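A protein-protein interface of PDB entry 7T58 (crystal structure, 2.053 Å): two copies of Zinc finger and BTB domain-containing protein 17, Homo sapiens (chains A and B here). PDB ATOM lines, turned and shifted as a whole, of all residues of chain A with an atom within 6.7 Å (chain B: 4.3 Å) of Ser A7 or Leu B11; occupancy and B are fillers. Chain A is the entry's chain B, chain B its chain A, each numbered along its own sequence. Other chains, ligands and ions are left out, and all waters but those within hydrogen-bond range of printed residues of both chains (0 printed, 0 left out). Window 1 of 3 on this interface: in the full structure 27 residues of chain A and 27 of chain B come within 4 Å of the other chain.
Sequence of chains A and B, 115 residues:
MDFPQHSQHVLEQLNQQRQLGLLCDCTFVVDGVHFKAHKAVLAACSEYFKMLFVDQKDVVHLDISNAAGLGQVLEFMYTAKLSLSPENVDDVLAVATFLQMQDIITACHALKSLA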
ATOM      1  N   PHE A   3      -0.607  37.289 -22.614  1.00  0.00           N
ATOM      2  CA  PHE A   3       0.074  36.631 -23.729  1.00  0.00           C
ATOM      3  C   PHE A   3      -0.231  35.141 -23.661  1.00  0.00           C
ATOM      4  O   PHE A   3       0.375  34.418 -22.847  1.00  0.00           O
ATOM      5  CB  PHE A   3       1.579  36.886 -23.676  1.00  0.00           C
ATOM      6  CG  PHE A   3       1.967  38.307 -23.999  1.00  0.00           C
ATOM      7  CD1 PHE A   3       1.670  39.340 -23.122  1.00  0.00           C
ATOM      8  CD2 PHE A   3       2.633  38.606 -25.177  1.00  0.00           C
ATOM      9  CE1 PHE A   3       2.026  40.644 -23.416  1.00  0.00           C
ATOM     10  CE2 PHE A   3       2.991  39.912 -25.477  1.00  0.00           C
ATOM     11  CZ  PHE A   3       2.687  40.931 -24.593  1.00  0.00           C
ATOM     12  N   PRO A   4      -1.152  34.631 -24.485  1.00  0.00           N
ATOM     13  CA  PRO A   4      -1.638  33.254 -24.289  1.00  0.00           C
ATOM     14  C   PRO A   4      -0.611  32.168 -24.583  1.00  0.00           C
ATOM     15  O   PRO A   4      -0.747  31.064 -24.042  1.00  0.00           O
ATOM     16  CB  PRO A   4      -2.832  33.162 -25.248  1.00  0.00           C
ATOM     17  CG  PRO A   4      -2.573  34.212 -26.279  1.00  0.00           C
ATOM     18  CD  PRO A   4      -1.881  35.331 -25.558  1.00  0.00           C
ATOM     19  N   GLN A   5       0.395  32.427 -25.418  1.00  0.00           N
ATOM     20  CA  GLN A   5       1.408  31.426 -25.735  1.00  0.00           C
ATOM     21  C   GLN A   5       2.692  31.588 -24.929  1.00  0.00           C
ATOM     22  O   GLN A   5       3.666  30.872 -25.195  1.00  0.00           O
ATOM     23  CB  GLN A   5       1.746  31.458 -27.231  1.00  0.00           C
ATOM     24  CG  GLN A   5       0.779  30.681 -28.111  1.00  0.00           C
ATOM     25  CD  GLN A   5      -0.528  31.414 -28.329  1.00  0.00           C
ATOM     26  OE1 GLN A   5      -0.596  32.636 -28.203  1.00  0.00           O
ATOM     27  NE2 GLN A   5      -1.574  30.670 -28.661  1.00  0.00           N
ATOM     28  N   HIS A   6       2.718  32.493 -23.949  1.00  0.00           N
ATOM     29  CA  HIS A   6       3.960  32.797 -23.243  1.00  0.00           C
ATOM     30  C   HIS A   6       4.493  31.580 -22.492  1.00  0.00           C
ATOM     31  O   HIS A   6       5.647  31.177 -22.680  1.00  0.00           O
ATOM     32  CB  HIS A   6       3.745  33.968 -22.286  1.00  0.00           C
ATOM     33  CG  HIS A   6       4.941  34.281 -21.446  1.00  0.00           C
ATOM     34  ND1 HIS A   6       6.109  34.785 -21.977  1.00  0.00           N
ATOM     35  CD2 HIS A   6       5.158  34.148 -20.116  1.00  0.00           C
ATOM     36  CE1 HIS A   6       6.991  34.959 -21.008  1.00  0.00           C
ATOM     37  NE2 HIS A   6       6.439  34.579 -19.870  1.00  0.00           N
ATOM     38  N   SER A   7       3.667  30.990 -21.620  1.00  0.00           N
ATOM     39  CA  SER A   7       4.134  29.867 -20.809  1.00  0.00           C
ATOM     40  C   SER A   7       4.618  28.713 -21.681  1.00  0.00           C
ATOM     41  O   SER A   7       5.623  28.065 -21.365  1.00  0.00           O
ATOM     42  CB  SER A   7       3.028  29.398 -19.865  1.00  0.00           C
ATOM     43  OG  SER A   7       2.015  28.702 -20.571  1.00  0.00           O
ATOM     44  N   GLN A   8       3.921  28.444 -22.790  1.00  0.00           N
ATOM     45  CA  GLN A   8       4.375  27.405 -23.707  1.00  0.00           C
ATOM     46  C   GLN A   8       5.727  27.757 -24.311  1.00  0.00           C
ATOM     47  O   GLN A   8       6.583  26.883 -24.492  1.00  0.00           O
ATOM     48  CB  GLN A   8       3.341  27.182 -24.814  1.00  0.00           C
ATOM     49  CG  GLN A   8       1.946  26.832 -24.317  1.00  0.00           C
ATOM     50  CD  GLN A   8       1.014  28.028 -24.285  1.00  0.00           C
ATOM     51  OE1 GLN A   8       1.050  28.838 -23.355  1.00  0.00           O
ATOM     52  NE2 GLN A   8       0.169  28.144 -25.308  1.00  0.00           N
ATOM     53  N   HIS A   9       5.940  29.035 -24.627  1.00  0.00           N
ATOM     54  CA  HIS A   9       7.194  29.437 -25.252  1.00  0.00           C
ATOM     55  C   HIS A   9       8.352  29.376 -24.264  1.00  0.00           C
ATOM     56  O   HIS A   9       9.478  29.023 -24.641  1.00  0.00           O
ATOM     57  CB  HIS A   9       7.054  30.838 -25.845  1.00  0.00           C
ATOM     58  CG  HIS A   9       6.184  30.889 -27.060  1.00  0.00           C
ATOM     59  ND1 HIS A   9       5.710  32.070 -27.586  1.00  0.00           N
ATOM     60  CD2 HIS A   9       5.709  29.904 -27.859  1.00  0.00           C
ATOM     61  CE1 HIS A   9       4.975  31.813 -28.653  1.00  0.00           C
ATOM     62  NE2 HIS A   9       4.960  30.504 -28.841  1.00  0.00           N
ATOM     63  N   VAL A  10       8.100  29.717 -22.997  1.00  0.00           N
ATOM     64  CA  VAL A  10       9.138  29.587 -21.978  1.00  0.00           C
ATOM     65  C   VAL A  10       9.560  28.131 -21.835  1.00  0.00           C
ATOM     66  O   VAL A  10      10.755  27.816 -21.776  1.00  0.00           O
ATOM     67  CB  VAL A  10       8.651  30.163 -20.635  1.00  0.00           C
ATOM     68  CG1 VAL A  10       9.593  29.760 -19.508  1.00  0.00           C
ATOM     69  CG2 VAL A  10       8.539  31.676 -20.716  1.00  0.00           C
ATOM     70  N   LEU A  11       8.587  27.220 -21.791  1.00  0.00           N
ATOM     71  CA  LEU A  11       8.901  25.811 -21.577  1.00  0.00           C
ATOM     72  C   LEU A  11       9.680  25.232 -22.749  1.00  0.00           C
ATOM     73  O   LEU A  11      10.593  24.423 -22.553  1.00  0.00           O
ATOM     74  CB  LEU A  11       7.620  25.014 -21.332  1.00  0.00           C
ATOM     75  CG  LEU A  11       7.843  23.559 -20.906  1.00  0.00           C
ATOM     76  CD1 LEU A  11       8.635  23.486 -19.607  1.00  0.00           C
ATOM     77  CD2 LEU A  11       6.523  22.812 -20.779  1.00  0.00           C
ATOM     78  N   GLU A  12       9.344  25.623 -23.979  1.00  0.00           N
ATOM     79  CA  GLU A  12      10.117  25.122 -25.110  1.00  0.00           C
ATOM     80  C   GLU A  12      11.538  25.669 -25.097  1.00  0.00           C
ATOM     81  O   GLU A  12      12.464  24.993 -25.561  1.00  0.00           O
ATOM     82  CB  GLU A  12       9.419  25.451 -26.430  1.00  0.00           C
ATOM     83  CG  GLU A  12      10.140  24.917 -27.670  1.00  0.00           C
ATOM     84  CD  GLU A  12      10.477  23.430 -27.583  1.00  0.00           C
ATOM     85  OE1 GLU A  12       9.713  22.664 -26.957  1.00  0.00           O
ATOM     86  OE2 GLU A  12      11.513  23.026 -28.153  1.00  0.00           O
ATOM     87  N   ALA A  44       9.437  21.838  -9.882  1.00  0.00           N
ATOM     88  CA  ALA A  44       8.116  22.310 -10.282  1.00  0.00           C
ATOM     89  C   ALA A  44       7.191  21.158 -10.648  1.00  0.00           C
ATOM     90  O   ALA A  44       5.970  21.273 -10.496  1.00  0.00           O
ATOM     91  CB  ALA A  44       8.238  23.282 -11.455  1.00  0.00           C
ATOM     92  N   SER B   7       2.318  23.774 -19.111  1.00  0.00           N
ATOM     93  CA  SER B   7       3.269  24.880 -19.188  1.00  0.00           C
ATOM     94  C   SER B   7       2.863  26.028 -18.271  1.00  0.00           C
ATOM     95  O   SER B   7       3.721  26.669 -17.653  1.00  0.00           O
ATOM     96  CB  SER B   7       3.401  25.367 -20.630  1.00  0.00           C
ATOM     97  OG  SER B   7       2.257  26.101 -21.027  1.00  0.00           O
ATOM     98  N   GLN B   8       1.562  26.310 -18.177  1.00  0.00           N
ATOM     99  CA  GLN B   8       1.090  27.296 -17.212  1.00  0.00           C
ATOM    100  C   GLN B   8       1.445  26.875 -15.790  1.00  0.00           C
ATOM    101  O   GLN B   8       1.930  27.683 -14.992  1.00  0.00           O
ATOM    102  CB  GLN B   8      -0.419  27.495 -17.363  1.00  0.00           C
ATOM    103  N   HIS B   9       1.234  25.596 -15.466  1.00  0.00           N
ATOM    104  CA  HIS B   9       1.521  25.106 -14.119  1.00  0.00           C
ATOM    105  C   HIS B   9       3.007  25.202 -13.788  1.00  0.00           C
ATOM    106  O   HIS B   9       3.379  25.542 -12.657  1.00  0.00           O
ATOM    107  CB  HIS B   9       1.026  23.666 -13.971  1.00  0.00           C
ATOM    108  CG  HIS B   9      -0.467  23.539 -13.967  1.00  0.00           C
ATOM    109  ND1 HIS B   9      -1.112  22.322 -14.017  1.00  0.00           N
ATOM    110  CD2 HIS B   9      -1.439  24.480 -13.912  1.00  0.00           C
ATOM    111  CE1 HIS B   9      -2.418  22.519 -13.998  1.00  0.00           C
ATOM    112  NE2 HIS B   9      -2.644  23.819 -13.933  1.00  0.00           N
ATOM    113  N   VAL B  10       3.873  24.900 -14.758  1.00  0.00           N
ATOM    114  CA  VAL B  10       5.314  25.017 -14.534  1.00  0.00           C
ATOM    115  C   VAL B  10       5.696  26.471 -14.278  1.00  0.00           C
ATOM    116  O   VAL B  10       6.454  26.779 -13.351  1.00  0.00           O
ATOM    117  CB  VAL B  10       6.096  24.431 -15.725  1.00  0.00           C
ATOM    118  CG1 VAL B  10       7.585  24.699 -15.567  1.00  0.00           C
ATOM    119  CG2 VAL B  10       5.842  22.939 -15.847  1.00  0.00           C
ATOM    120  N   LEU B  11       5.173  27.388 -15.094  1.00  0.00           N
ATOM    121  CA  LEU B  11       5.510  28.799 -14.925  1.00  0.00           C
ATOM    122  C   LEU B  11       4.969  29.344 -13.608  1.00  0.00           C
ATOM    123  O   LEU B  11       5.628  30.159 -12.951  1.00  0.00           O
ATOM    124  CB  LEU B  11       4.979  29.615 -16.101  1.00  0.00           C
ATOM    125  CG  LEU B  11       5.510  31.047 -16.162  1.00  0.00           C
ATOM    126  CD1 LEU B  11       7.027  31.033 -16.220  1.00  0.00           C
ATOM    127  CD2 LEU B  11       4.925  31.788 -17.356  1.00  0.00           C
ATOM    128  N   GLU B  12       3.772  28.907 -13.206  1.00  0.00           N
ATOM    129  CA  GLU B  12       3.246  29.300 -11.901  1.00  0.00           C
ATOM    130  C   GLU B  12       4.144  28.806 -10.774  1.00  0.00           C
ATOM    131  O   GLU B  12       4.359  29.516  -9.784  1.00  0.00           O
ATOM    132  CB  GLU B  12       1.820  28.774 -11.729  1.00  0.00           C
ATOM    133  CG  GLU B  12       0.802  29.467 -12.626  1.00  0.00           C
ATOM    134  CD  GLU B  12      -0.516  28.717 -12.716  1.00  0.00           C
ATOM    135  OE1 GLU B  12      -0.677  27.696 -12.014  1.00  0.00           O
ATOM    136  OE2 GLU B  12      -1.390  29.151 -13.497  1.00  0.00           O
ATOM    137  N   GLN B  13       4.687  27.595 -10.911  1.00  0.00           N
ATOM    138  CA  GLN B  13       5.602  27.077  -9.900  1.00  0.00           C
ATOM    139  C   GLN B  13       6.912  27.854  -9.889  1.00  0.00           C
ATOM    140  O   GLN B  13       7.487  28.094  -8.821  1.00  0.00           O
ATOM    141  CB  GLN B  13       5.862  25.592 -10.139  1.00  0.00           C
ATOM    142  CG  GLN B  13       4.752  24.684  -9.647  1.00  0.00           C
ATOM    143  CD  GLN B  13       4.672  24.640  -8.136  1.00  0.00           C
ATOM    144  OE1 GLN B  13       5.664  24.367  -7.457  1.00  0.00           O
ATOM    145  NE2 GLN B  13       3.489  24.918  -7.599  1.00  0.00           N
ATOM    146  N   LEU B  14       7.403  28.250 -11.065  1.00  0.00           N
ATOM    147  CA  LEU B  14       8.605  29.076 -11.117  1.00  0.00           C
ATOM    148  C   LEU B  14       8.353  30.444 -10.495  1.00  0.00           C
ATOM    149  O   LEU B  14       9.229  30.996  -9.820  1.00  0.00           O
ATOM    150  CB  LEU B  14       9.079  29.216 -12.563  1.00  0.00           C
ATOM    151  CG  LEU B  14       9.533  27.911 -13.210  1.00  0.00           C
ATOM    152  CD1 LEU B  14       9.813  28.098 -14.698  1.00  0.00           C
ATOM    153  CD2 LEU B  14      10.762  27.381 -12.485  1.00  0.00           C
ATOM    154  N   ASN B  15       7.157  31.000 -10.707  1.00  0.00           N
ATOM    155  CA  ASN B  15       6.818  32.283 -10.101  1.00  0.00           C
ATOM    156  C   ASN B  15       6.799  32.185  -8.580  1.00  0.00           C
ATOM    157  O   ASN B  15       7.285  33.087  -7.888  1.00  0.00           O
ATOM    158  CB  ASN B  15       5.466  32.767 -10.623  1.00  0.00           C
ATOM    159  CG  ASN B  15       5.220  34.235 -10.332  1.00  0.00           C
ATOM    160  OD1 ASN B  15       6.160  35.014 -10.174  1.00  0.00           O
ATOM    161  ND2 ASN B  15       3.953  34.622 -10.272  1.00  0.00           N
ATOM    162  N   MET B  77       7.721  37.981 -17.519  1.00  0.00           N
ATOM    163  CA  MET B  77       8.359  36.691 -17.772  1.00  0.00           C
ATOM    164  C   MET B  77       7.743  35.588 -16.924  1.00  0.00           C
ATOM    165  O   MET B  77       7.556  34.461 -17.397  1.00  0.00           O
ATOM    166  CB  MET B  77       9.860  36.775 -17.493  1.00  0.00           C
ATOM    167  CG  MET B  77      10.630  37.759 -18.355  1.00  0.00           C
ATOM    168  SD  MET B  77      12.387  37.709 -17.942  1.00  0.00           S
ATOM    169  CE  MET B  77      13.047  38.951 -19.053  1.00  0.00           C
ATOM    170  N   TYR B  78       7.423  35.892 -15.670  1.00  0.00           N
ATOM    171  CA  TYR B  78       6.972  34.880 -14.729  1.00  0.00           C
ATOM    172  C   TYR B  78       5.457  34.729 -14.668  1.00  0.00           C
ATOM    173  O   TYR B  78       4.976  33.792 -14.023  1.00  0.00           O
ATOM    174  CB  TYR B  78       7.508  35.194 -13.328  1.00  0.00           C
ATOM    175  CG  TYR B  78       8.948  34.778 -13.121  1.00  0.00           C
ATOM    176  CD1 TYR B  78       9.263  33.490 -12.712  1.00  0.00           C
ATOM    177  CD2 TYR B  78       9.992  35.670 -13.338  1.00  0.00           C
ATOM    178  CE1 TYR B  78      10.573  33.100 -12.518  1.00  0.00           C
ATOM    179  CE2 TYR B  78      11.310  35.287 -13.149  1.00  0.00           C
ATOM    180  CZ  TYR B  78      11.593  33.998 -12.742  1.00  0.00           C
ATOM    181  OH  TYR B  78      12.897  33.603 -12.546  1.00  0.00           O
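Hydrophobic or aromatic side chains of chain A that line the printed part of chain B: His A6 and Ala A44.
Of the 11 printed residues of chain B, 5 touch a printed residue of chain A.
Printed residues of chain B that touch a printed residue of chain A: Ser B7, Gln B8, Leu B11, Gln B13 and Met B77.
Hydrophobic or aromatic side chains of chain B that line the printed part of chain A: Leu B11.
Among the printed residues, 7 pairs touch across the chains.
Among the printed residues, no Asp or Glu carboxylate lies within 4 Å of a Lys or Arg side-chain nitrogen of the other chain.
Among the printed residues, pairs that only touch across the chains: Ala A44 with Gln B13, His A6 with Leu B11 and Ser A7 with Leu B11.
Ser B7 touches its own counterpart, Ser A7.
Ser A7 touches Gln B8, and with the chains exchanged Gln A8 touches Ser B7.
Ser A7 touches Leu B11, but with the chains exchanged Leu A11 does not touch Ser B7 (4.04 Å).
Positions printed for both chains: 7, 8, 9, 10, 11 and 12.
The side-chain amide oxygen of Gln A8 lies close to the backbone carbonyl oxygen of Pro A4, 2.9 Å away.
OE1 of Gln A8 sits at hydrogen-bond distance from OG of Ser A7.
The side-chain hydroxyl of Ser B7 sits at hydrogen-bond distance from the side-chain hydroxyl of Ser A7 (2.7 Å).
The side-chain hydroxyl (OG) of Ser B7 is in hydrogen-bond range of the backbone NH (N) of Gln A8, 3.4 Å away.
N of Gln B8 is in hydrogen-bond range of OG of Ser A7 (3.4 Å).
The backbone carbonyl oxygen (O) of Met B77 is in hydrogen-bond range of a ring nitrogen (NE2) of His A6 (2.7 Å).
Of chain B, only Ser B7, Gln B8 and Leu B11 come within 4 Å of Ser A7.
Of chain A, only His A6 (3.6 Å) and Ser A7 (3.95 Å) come within 4 Å of Leu B11.
Of the printed residues of chain B, Ala A44 touches Gln B13.
Printed residues of chain A within 4 Å of Gln B13: Ala A44.
The nearest printed residue of chain A that does not touch Ser B7 is Leu A11 (4.04 Å).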
